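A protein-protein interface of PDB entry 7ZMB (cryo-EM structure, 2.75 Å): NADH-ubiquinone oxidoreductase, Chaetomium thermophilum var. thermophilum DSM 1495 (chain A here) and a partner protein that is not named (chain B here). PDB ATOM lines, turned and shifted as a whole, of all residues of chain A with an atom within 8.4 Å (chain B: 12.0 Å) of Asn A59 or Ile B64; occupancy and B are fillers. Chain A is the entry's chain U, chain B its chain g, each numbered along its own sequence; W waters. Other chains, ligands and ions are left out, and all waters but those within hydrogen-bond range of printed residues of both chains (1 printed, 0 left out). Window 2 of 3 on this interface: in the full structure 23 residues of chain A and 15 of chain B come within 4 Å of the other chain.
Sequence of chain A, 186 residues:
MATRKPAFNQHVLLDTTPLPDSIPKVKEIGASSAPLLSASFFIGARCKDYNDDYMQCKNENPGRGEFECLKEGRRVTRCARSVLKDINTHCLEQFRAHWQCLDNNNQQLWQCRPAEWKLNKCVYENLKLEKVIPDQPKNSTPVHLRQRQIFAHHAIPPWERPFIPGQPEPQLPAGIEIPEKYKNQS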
ATOM      1  N   ASN A  51      28.051  32.394 -11.552  1.00  0.00           N
ATOM      2  CA  ASN A  51      28.558  31.013 -11.336  1.00  0.00           C
ATOM      3  C   ASN A  51      27.368  30.060 -11.339  1.00  0.00           C
ATOM      4  O   ASN A  51      27.441  29.028 -12.026  1.00  0.00           O
ATOM      5  CB  ASN A  51      29.265  30.880  -9.989  1.00  0.00           C
ATOM      6  CG  ASN A  51      30.603  31.584  -9.935  1.00  0.00           C
ATOM      7  OD1 ASN A  51      31.060  32.138 -10.931  1.00  0.00           O
ATOM      8  ND2 ASN A  51      31.243  31.563  -8.777  1.00  0.00           N
ATOM      9  N   ASP A  52      26.305  30.412 -10.621  1.00  0.00           N
ATOM     10  CA  ASP A  52      25.098  29.548 -10.519  1.00  0.00           C
ATOM     11  C   ASP A  52      24.390  29.453 -11.869  1.00  0.00           C
ATOM     12  O   ASP A  52      23.738  28.426 -12.109  1.00  0.00           O
ATOM     13  CB  ASP A  52      24.184  29.992  -9.380  1.00  0.00           C
ATOM     14  CG  ASP A  52      24.760  29.749  -7.997  1.00  0.00           C
ATOM     15  OD1 ASP A  52      25.802  29.076  -7.902  1.00  0.00           O
ATOM     16  OD2 ASP A  52      24.155  30.237  -7.023  1.00  0.00           O
ATOM     17  N   ASP A  53      24.549  30.452 -12.732  1.00  0.00           N
ATOM     18  CA  ASP A  53      23.818  30.482 -14.024  1.00  0.00           C
ATOM     19  C   ASP A  53      24.553  29.581 -15.012  1.00  0.00           C
ATOM     20  O   ASP A  53      23.875  28.851 -15.749  1.00  0.00           O
ATOM     21  CB  ASP A  53      23.708  31.898 -14.579  1.00  0.00           C
ATOM     22  CG  ASP A  53      22.613  32.069 -15.615  1.00  0.00           C
ATOM     23  OD1 ASP A  53      21.566  31.418 -15.468  1.00  0.00           O
ATOM     24  OD2 ASP A  53      22.822  32.856 -16.557  1.00  0.00           O
ATOM     25  N   TYR A  54      25.884  29.665 -15.033  1.00  0.00           N
ATOM     26  CA  TYR A  54      26.712  28.773 -15.889  1.00  0.00           C
ATOM     27  C   TYR A  54      26.349  27.310 -15.632  1.00  0.00           C
ATOM     28  O   TYR A  54      26.013  26.606 -16.584  1.00  0.00           O
ATOM     29  CB  TYR A  54      28.195  29.123 -15.747  1.00  0.00           C
ATOM     30  CG  TYR A  54      29.117  28.352 -16.652  1.00  0.00           C
ATOM     31  CD1 TYR A  54      28.947  28.386 -18.023  1.00  0.00           C
ATOM     32  CD2 TYR A  54      30.156  27.594 -16.143  1.00  0.00           C
ATOM     33  CE1 TYR A  54      29.784  27.685 -18.870  1.00  0.00           C
ATOM     34  CE2 TYR A  54      31.005  26.886 -16.977  1.00  0.00           C
ATOM     35  CZ  TYR A  54      30.815  26.935 -18.345  1.00  0.00           C
ATOM     36  OH  TYR A  54      31.628  26.248 -19.193  1.00  0.00           O
ATOM     37  N   MET A  55      26.467  26.866 -14.387  1.00  0.00           N
ATOM     38  CA  MET A  55      26.232  25.453 -13.997  1.00  0.00           C
ATOM     39  C   MET A  55      24.794  24.989 -14.283  1.00  0.00           C
ATOM     40  O   MET A  55      24.645  23.819 -14.638  1.00  0.00           O
ATOM     41  CB  MET A  55      26.596  25.274 -12.520  1.00  0.00           C
ATOM     42  CG  MET A  55      27.980  25.771 -12.174  1.00  0.00           C
ATOM     43  SD  MET A  55      29.273  24.734 -12.875  1.00  0.00           S
ATOM     44  CE  MET A  55      29.078  23.257 -11.882  1.00  0.00           C
ATOM     45  N   GLN A  56      23.793  25.865 -14.137  1.00  0.00           N
ATOM     46  CA  GLN A  56      22.369  25.525 -14.391  1.00  0.00           C
ATOM     47  C   GLN A  56      22.167  25.433 -15.901  1.00  0.00           C
ATOM     48  O   GLN A  56      21.379  24.572 -16.328  1.00  0.00           O
ATOM     49  CB  GLN A  56      21.424  26.559 -13.799  1.00  0.00           C
ATOM     50  CG  GLN A  56      21.078  26.308 -12.340  1.00  0.00           C
ATOM     51  CD  GLN A  56      20.304  27.460 -11.753  1.00  0.00           C
ATOM     52  OE1 GLN A  56      20.352  28.580 -12.250  1.00  0.00           O
ATOM     53  NE2 GLN A  56      19.582  27.188 -10.681  1.00  0.00           N
ATOM     54  N   CYS A  57      22.896  26.230 -16.673  1.00  0.00           N
ATOM     55  CA  CYS A  57      22.844  26.112 -18.147  1.00  0.00           C
ATOM     56  C   CYS A  57      23.412  24.753 -18.572  1.00  0.00           C
ATOM     57  O   CYS A  57      22.800  24.107 -19.426  1.00  0.00           O
ATOM     58  CB  CYS A  57      23.646  27.243 -18.783  1.00  0.00           C
ATOM     59  SG  CYS A  57      23.609  27.251 -20.594  1.00  0.00           S
ATOM     60  N   LYS A  58      24.552  24.346 -18.008  1.00  0.00           N
ATOM     61  CA  LYS A  58      25.184  23.054 -18.380  1.00  0.00           C
ATOM     62  C   LYS A  58      24.250  21.899 -18.005  1.00  0.00           C
ATOM     63  O   LYS A  58      24.139  20.968 -18.805  1.00  0.00           O
ATOM     64  CB  LYS A  58      26.611  22.978 -17.833  1.00  0.00           C
ATOM     65  CG  LYS A  58      27.562  24.030 -18.381  1.00  0.00           C
ATOM     66  CD  LYS A  58      29.000  23.777 -18.011  1.00  0.00           C
ATOM     67  CE  LYS A  58      29.548  22.502 -18.615  1.00  0.00           C
ATOM     68  NZ  LYS A  58      30.966  22.302 -18.244  1.00  0.00           N
ATOM     69  N   ASN A  59      23.577  21.991 -16.859  1.00  0.00           N
ATOM     70  CA  ASN A  59      22.616  20.950 -16.407  1.00  0.00           C
ATOM     71  C   ASN A  59      21.334  21.073 -17.239  1.00  0.00           C
ATOM     72  O   ASN A  59      20.535  20.134 -17.195  1.00  0.00           O
ATOM     73  CB  ASN A  59      22.343  21.051 -14.908  1.00  0.00           C
ATOM     74  CG  ASN A  59      23.352  20.333 -14.044  1.00  0.00           C
ATOM     75  OD1 ASN A  59      24.510  20.205 -14.417  1.00  0.00           O
ATOM     76  ND2 ASN A  59      22.924  19.870 -12.883  1.00  0.00           N
ATOM     77  N   GLU A  60      21.173  22.155 -18.009  1.00  0.00           N
ATOM     78  CA  GLU A  60      20.031  22.270 -18.901  1.00  0.00           C
ATOM     79  C   GLU A  60      20.309  21.716 -20.288  1.00  0.00           C
ATOM     80  O   GLU A  60      19.364  21.481 -21.043  1.00  0.00           O
ATOM     81  CB  GLU A  60      19.608  23.729 -19.013  1.00  0.00           C
ATOM     82  CG  GLU A  60      18.151  23.948 -19.325  1.00  0.00           C
ATOM     83  CD  GLU A  60      17.788  25.417 -19.336  1.00  0.00           C
ATOM     84  OE1 GLU A  60      17.241  25.891 -20.354  1.00  0.00           O
ATOM     85  OE2 GLU A  60      18.059  26.099 -18.327  1.00  0.00           O
ATOM     86  N   ASN A  61      21.574  21.501 -20.640  1.00  0.00           N
ATOM     87  CA  ASN A  61      21.961  20.900 -21.916  1.00  0.00           C
ATOM     88  C   ASN A  61      22.951  19.776 -21.650  1.00  0.00           C
ATOM     89  O   ASN A  61      24.166  19.950 -21.815  1.00  0.00           O
ATOM     90  CB  ASN A  61      22.565  21.937 -22.862  1.00  0.00           C
ATOM     91  CG  ASN A  61      21.757  23.206 -22.926  1.00  0.00           C
ATOM     92  OD1 ASN A  61      22.067  24.186 -22.255  1.00  0.00           O
ATOM     93  ND2 ASN A  61      20.716  23.199 -23.743  1.00  0.00           N
ATOM     94  N   PRO A  62      22.469  18.606 -21.236  1.00  0.00           N
ATOM     95  CA  PRO A  62      23.388  17.506 -20.909  1.00  0.00           C
ATOM     96  C   PRO A  62      24.121  16.996 -22.142  1.00  0.00           C
ATOM     97  O   PRO A  62      23.512  16.699 -23.170  1.00  0.00           O
ATOM     98  CB  PRO A  62      22.463  16.439 -20.315  1.00  0.00           C
ATOM     99  CG  PRO A  62      21.275  17.208 -19.834  1.00  0.00           C
ATOM    100  CD  PRO A  62      21.091  18.302 -20.834  1.00  0.00           C
ATOM    101  N   GLY A  63      25.443  16.897 -22.025  1.00  0.00           N
ATOM    102  CA  GLY A  63      26.292  16.475 -23.111  1.00  0.00           C
ATOM    103  C   GLY A  63      26.666  17.561 -24.086  1.00  0.00           C
ATOM    104  O   GLY A  63      27.460  17.304 -24.994  1.00  0.00           O
ATOM    105  N   ARG A  64      26.122  18.765 -23.931  1.00  0.00           N
ATOM    106  CA  ARG A  64      26.309  19.857 -24.876  1.00  0.00           C
ATOM    107  C   ARG A  64      26.664  21.151 -24.161  1.00  0.00           C
ATOM    108  O   ARG A  64      26.580  22.226 -24.758  1.00  0.00           O
ATOM    109  CB  ARG A  64      25.046  20.066 -25.713  1.00  0.00           C
ATOM    110  CG  ARG A  64      24.629  18.890 -26.554  1.00  0.00           C
ATOM    111  CD  ARG A  64      25.414  18.855 -27.820  1.00  0.00           C
ATOM    112  NE  ARG A  64      25.730  20.197 -28.288  1.00  0.00           N
ATOM    113  CZ  ARG A  64      26.581  20.459 -29.272  1.00  0.00           C
ATOM    114  NH1 ARG A  64      27.200  19.466 -29.890  1.00  0.00           N
ATOM    115  NH2 ARG A  64      26.813  21.708 -29.638  1.00  0.00           N
ATOM    116  N   GLY A  65      26.943  21.075 -22.860  1.00  0.00           N
ATOM    117  CA  GLY A  65      27.177  22.309 -22.089  1.00  0.00           C
ATOM    118  C   GLY A  65      28.365  23.078 -22.615  1.00  0.00           C
ATOM    119  O   GLY A  65      28.295  24.316 -22.645  1.00  0.00           O
ATOM    120  N   CYS A  69      26.770  26.797 -23.687  1.00  0.00           N
ATOM    121  CA  CYS A  69      26.708  27.758 -22.556  1.00  0.00           C
ATOM    122  C   CYS A  69      27.916  28.702 -22.577  1.00  0.00           C
ATOM    123  O   CYS A  69      28.357  29.119 -21.496  1.00  0.00           O
ATOM    124  CB  CYS A  69      26.591  27.016 -21.232  1.00  0.00           C
ATOM    125  SG  CYS A  69      25.107  25.982 -21.136  1.00  0.00           S
ATOM    126  N   ILE B  58      29.156  18.133   4.547  1.00  0.00           N
ATOM    127  CA  ILE B  58      30.021  19.079   3.775  1.00  0.00           C
ATOM    128  C   ILE B  58      29.832  18.855   2.268  1.00  0.00           C
ATOM    129  O   ILE B  58      29.577  17.711   1.869  1.00  0.00           O
ATOM    130  CB  ILE B  58      31.491  18.976   4.221  1.00  0.00           C
ATOM    131  CG1 ILE B  58      32.160  17.686   3.741  1.00  0.00           C
ATOM    132  CG2 ILE B  58      31.605  19.151   5.727  1.00  0.00           C
ATOM    133  CD1 ILE B  58      33.585  17.876   3.286  1.00  0.00           C
ATOM    134  N   PRO B  59      29.885  19.897   1.415  1.00  0.00           N
ATOM    135  CA  PRO B  59      29.635  19.712  -0.019  1.00  0.00           C
ATOM    136  C   PRO B  59      30.729  18.853  -0.686  1.00  0.00           C
ATOM    137  O   PRO B  59      31.886  19.109  -0.467  1.00  0.00           O
ATOM    138  CB  PRO B  59      29.572  21.154  -0.541  1.00  0.00           C
ATOM    139  CG  PRO B  59      30.369  21.967   0.453  1.00  0.00           C
ATOM    140  CD  PRO B  59      30.142  21.287   1.785  1.00  0.00           C
ATOM    141  N   LEU B  60      30.339  17.837  -1.454  1.00  0.00           N
ATOM    142  CA  LEU B  60      31.315  16.927  -2.109  1.00  0.00           C
ATOM    143  C   LEU B  60      31.057  16.979  -3.609  1.00  0.00           C
ATOM    144  O   LEU B  60      31.891  16.462  -4.361  1.00  0.00           O
ATOM    145  CB  LEU B  60      31.201  15.525  -1.509  1.00  0.00           C
ATOM    146  CG  LEU B  60      31.634  15.404  -0.050  1.00  0.00           C
ATOM    147  CD1 LEU B  60      31.567  13.966   0.426  1.00  0.00           C
ATOM    148  CD2 LEU B  60      33.038  15.951   0.136  1.00  0.00           C
ATOM    149  N   THR B  61      30.041  17.726  -4.019  1.00  0.00           N
ATOM    150  CA  THR B  61      29.789  17.988  -5.458  1.00  0.00           C
ATOM    151  C   THR B  61      29.257  19.419  -5.507  1.00  0.00           C
ATOM    152  O   THR B  61      28.803  19.907  -4.461  1.00  0.00           O
ATOM    153  CB  THR B  61      28.749  17.025  -6.050  1.00  0.00           C
ATOM    154  OG1 THR B  61      28.730  17.176  -7.468  1.00  0.00           O
ATOM    155  CG2 THR B  61      27.356  17.245  -5.504  1.00  0.00           C
ATOM    156  N   TYR B  62      29.445  20.106  -6.631  1.00  0.00           N
ATOM    157  CA  TYR B  62      28.932  21.491  -6.756  1.00  0.00           C
ATOM    158  C   TYR B  62      27.440  21.454  -6.433  1.00  0.00           C
ATOM    159  O   TYR B  62      26.712  20.608  -6.969  1.00  0.00           O
ATOM    160  CB  TYR B  62      29.177  22.056  -8.156  1.00  0.00           C
ATOM    161  CG  TYR B  62      28.937  23.540  -8.285  1.00  0.00           C
ATOM    162  CD1 TYR B  62      27.658  24.052  -8.435  1.00  0.00           C
ATOM    163  CD2 TYR B  62      29.990  24.436  -8.255  1.00  0.00           C
ATOM    164  CE1 TYR B  62      27.429  25.413  -8.535  1.00  0.00           C
ATOM    165  CE2 TYR B  62      29.781  25.799  -8.368  1.00  0.00           C
ATOM    166  CZ  TYR B  62      28.496  26.290  -8.505  1.00  0.00           C
ATOM    167  OH  TYR B  62      28.295  27.634  -8.618  1.00  0.00           O
ATOM    168  N   PRO B  63      26.952  22.361  -5.567  1.00  0.00           N
ATOM    169  CA  PRO B  63      25.552  22.363  -5.194  1.00  0.00           C
ATOM    170  C   PRO B  63      24.812  23.123  -6.296  1.00  0.00           C
ATOM    171  O   PRO B  63      24.888  24.323  -6.335  1.00  0.00           O
ATOM    172  CB  PRO B  63      25.534  23.167  -3.886  1.00  0.00           C
ATOM    173  CG  PRO B  63      26.991  23.398  -3.534  1.00  0.00           C
ATOM    174  CD  PRO B  63      27.728  23.368  -4.851  1.00  0.00           C
ATOM    175  N   ILE B  64      24.119  22.386  -7.156  1.00  0.00           N
ATOM    176  CA  ILE B  64      23.398  23.040  -8.279  1.00  0.00           C
ATOM    177  C   ILE B  64      22.151  23.687  -7.678  1.00  0.00           C
ATOM    178  O   ILE B  64      21.383  22.947  -7.042  1.00  0.00           O
ATOM    179  CB  ILE B  64      23.072  22.078  -9.439  1.00  0.00           C
ATOM    180  CG1 ILE B  64      24.337  21.465 -10.043  1.00  0.00           C
ATOM    181  CG2 ILE B  64      22.227  22.781 -10.488  1.00  0.00           C
ATOM    182  CD1 ILE B  64      25.121  22.418 -10.905  1.00  0.00           C
ATOM    183  N   PRO B  65      21.917  25.019  -7.798  1.00  0.00           N
ATOM    184  CA  PRO B  65      20.720  25.584  -7.208  1.00  0.00           C
ATOM    185  C   PRO B  65      19.427  25.057  -7.853  1.00  0.00           C
ATOM    186  O   PRO B  65      19.471  24.794  -9.033  1.00  0.00           O
ATOM    187  CB  PRO B  65      20.908  27.079  -7.491  1.00  0.00           C
ATOM    188  CG  PRO B  65      22.385  27.243  -7.695  1.00  0.00           C
ATOM    189  CD  PRO B  65      22.760  26.004  -8.469  1.00  0.00           C
ATOM    190  N   PRO B  66      18.285  24.861  -7.142  1.00  0.00           N
ATOM    191  CA  PRO B  66      17.042  24.503  -7.825  1.00  0.00           C
ATOM    192  C   PRO B  66      16.279  25.735  -8.294  1.00  0.00           C
ATOM    193  O   PRO B  66      16.516  26.860  -7.848  1.00  0.00           O
ATOM    194  CB  PRO B  66      16.260  23.755  -6.739  1.00  0.00           C
ATOM    195  CG  PRO B  66      16.709  24.405  -5.462  1.00  0.00           C
ATOM    196  CD  PRO B  66      18.099  24.970  -5.686  1.00  0.00           C
ATOM    197  N   GLY B  67      15.348  25.497  -9.214  1.00  0.00           N
ATOM    198  CA  GLY B  67      14.510  26.551  -9.735  1.00  0.00           C
ATOM    199  C   GLY B  67      14.985  27.079 -11.074  1.00  0.00           C
ATOM    200  O   GLY B  67      16.053  26.714 -11.572  1.00  0.00           O
ATOM    201  N   PRO B  68      14.188  27.950 -11.685  1.00  0.00           N
ATOM    202  CA  PRO B  68      14.553  28.494 -12.996  1.00  0.00           C
ATOM    203  C   PRO B  68      15.723  29.462 -12.903  1.00  0.00           C
ATOM    204  O   PRO B  68      16.010  30.042 -11.855  1.00  0.00           O
ATOM    205  CB  PRO B  68      13.277  29.210 -13.448  1.00  0.00           C
ATOM    206  CG  PRO B  68      12.592  29.581 -12.179  1.00  0.00           C
ATOM    207  CD  PRO B  68      12.908  28.489 -11.195  1.00  0.00           C
ATOM    208  N   ARG B  69      16.402  29.630 -14.035  1.00  0.00           N
ATOM    209  CA  ARG B  69      17.538  30.537 -14.104  1.00  0.00           C
ATOM    210  C   ARG B  69      17.084  31.978 -13.895  1.00  0.00           C
ATOM    211  O   ARG B  69      15.954  32.351 -14.213  1.00  0.00           O
ATOM    212  CB  ARG B  69      18.259  30.383 -15.440  1.00  0.00           C
ATOM    213  CG  ARG B  69      19.006  29.061 -15.571  1.00  0.00           C
ATOM    214  CD  ARG B  69      19.244  28.700 -17.016  1.00  0.00           C
ATOM    215  NE  ARG B  69      20.283  29.513 -17.628  1.00  0.00           N
ATOM    216  CZ  ARG B  69      20.764  29.306 -18.847  1.00  0.00           C
ATOM    217  NH1 ARG B  69      21.712  30.098 -19.325  1.00  0.00           N
ATOM    218  NH2 ARG B  69      20.299  28.311 -19.589  1.00  0.00           N
ATOM    219  N   LYS B  70      17.985  32.791 -13.350  1.00  0.00           N
ATOM    220  CA  LYS B  70      17.605  34.056 -12.735  1.00  0.00           C
ATOM    221  C   LYS B  70      17.516  35.222 -13.712  1.00  0.00           C
ATOM    222  O   LYS B  70      17.221  36.338 -13.271  1.00  0.00           O
ATOM    223  CB  LYS B  70      18.581  34.400 -11.609  1.00  0.00           C
ATOM    224  CG  LYS B  70      18.288  33.678 -10.307  1.00  0.00           C
ATOM    225  CD  LYS B  70      19.498  33.661  -9.389  1.00  0.00           C
ATOM    226  CE  LYS B  70      19.572  34.921  -8.548  1.00  0.00           C
ATOM    227  NZ  LYS B  70      18.611  34.886  -7.413  1.00  0.00           N
HETATM  228  O   HOH W   1      30.106  29.436  -6.611  1.00  0.00           O
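Printed residues of chain B that touch a printed residue of chain A: Tyr B62, Ile B64, Pro B65, Gly B67 and Arg B69.
Hydrophobic or aromatic side chains of chain B that line the printed part of chain A: Tyr B62, Ile B64 and Pro B65.
Of the 16 printed residues of chain A, 8 touch a printed residue of chain B.
Printed residues of chain A that touch a printed residue of chain B: Asn A51, Asp A52, Asp A53, Met A55, Gln A56, Cys A57, Asn A59 and Glu A60.
Hydrophobic or aromatic side chains of chain A within 4 Å of the printed part of chain B: Met A55.
Among the printed residues, Asp or Glu carboxylates within 4 Å of a Lys or Arg side-chain nitrogen of the other chain: Asp A53 with Arg B69 (3.2 Å) and Glu A60 with Arg B69 (3.4 Å).
Of the printed residues of chain B, Asn A51 touches Tyr B62.
Of the printed residues of chain B, Asp A52 touches Tyr B62 (3.0 Å) and Pro B65 (3.5 Å).
Of the printed residues of chain B, Asp A53 touches Arg B69.
Met A55 touches just these residues of chain B: Tyr B62 and Ile B64.
Of the printed residues of chain B, Gln A56 touches Pro B65 (2.9 Å), Gly B67 (3.7 Å) and Arg B69 (3.6 Å).
Cys A57 touches just one residue of chain B: Arg B69 (3.5 Å).
No residue of chain B comes within 4 Å of Lys A58.
Asn A59 touches just one residue of chain B: Ile B64.
Of chain B, only Arg B69 (3.1 Å) comes within 4 Å of Glu A60.
No residue of chain B comes within 4 Å of Pro A62.
No residue of chain B comes within 4 Å of Gly A65.
Of the printed residues of chain A, Tyr B62 touches Asn A51 (3.7 Å), Asp A52 (3.0 Å) and Met A55 (3.6 Å).
Of chain A, only Met A55 and Asn A59 come within 4 Å of Ile B64.
Of the printed residues of chain A, Arg B69 touches Asp A53, Gln A56, Cys A57 and Glu A60.
The nearest residue of chain A that does not touch Ile B64 is Gln A56 (4.1 Å).
OD1 of Asp A53 is in salt-bridge range of NE of Arg B69 (3.2 Å).
NH2 of Arg B69 lies within salt-bridge range of OE2 of Glu A60 (3.4 Å).
The side-chain amide nitrogen of Gln A56 sits at hydrogen-bond distance from the backbone carbonyl oxygen of Pro B65.
The guanidinium group of Arg B69 lies close to the side-chain sulfur of Cys A57.
OD1 of Asp A52 sits at hydrogen-bond distance from OH of Tyr B62 (3.0 Å).
The side-chain amide oxygen of Gln A56 lies close to the backbone carbonyl oxygen of Asp A52, 3.4 Å away.
O of Cys A57 lies close to OD1 of Asn A61 (2.9 Å).
The side-chain sulfur (SG) of Cys A57 forms a disulfide with the side-chain sulfur (SG) of Cys A69, at 2.0 Å.
Among the printed residues, merely in contact across the chains: Asn A51 with Tyr B62, Asp A52 with Pro B65, Met A55 with Tyr B62, Met A55 with Ile B64, Gln A56 with Gly B67, Gln A56 with Arg B69 and Asn A59 with Ile B64.
Water W1 bridges the side-chain amide nitrogen (ND2) of Asn A51 (3.2 Å) and the side-chain hydroxyl (OH) of Tyr B62 (3.2 Å).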
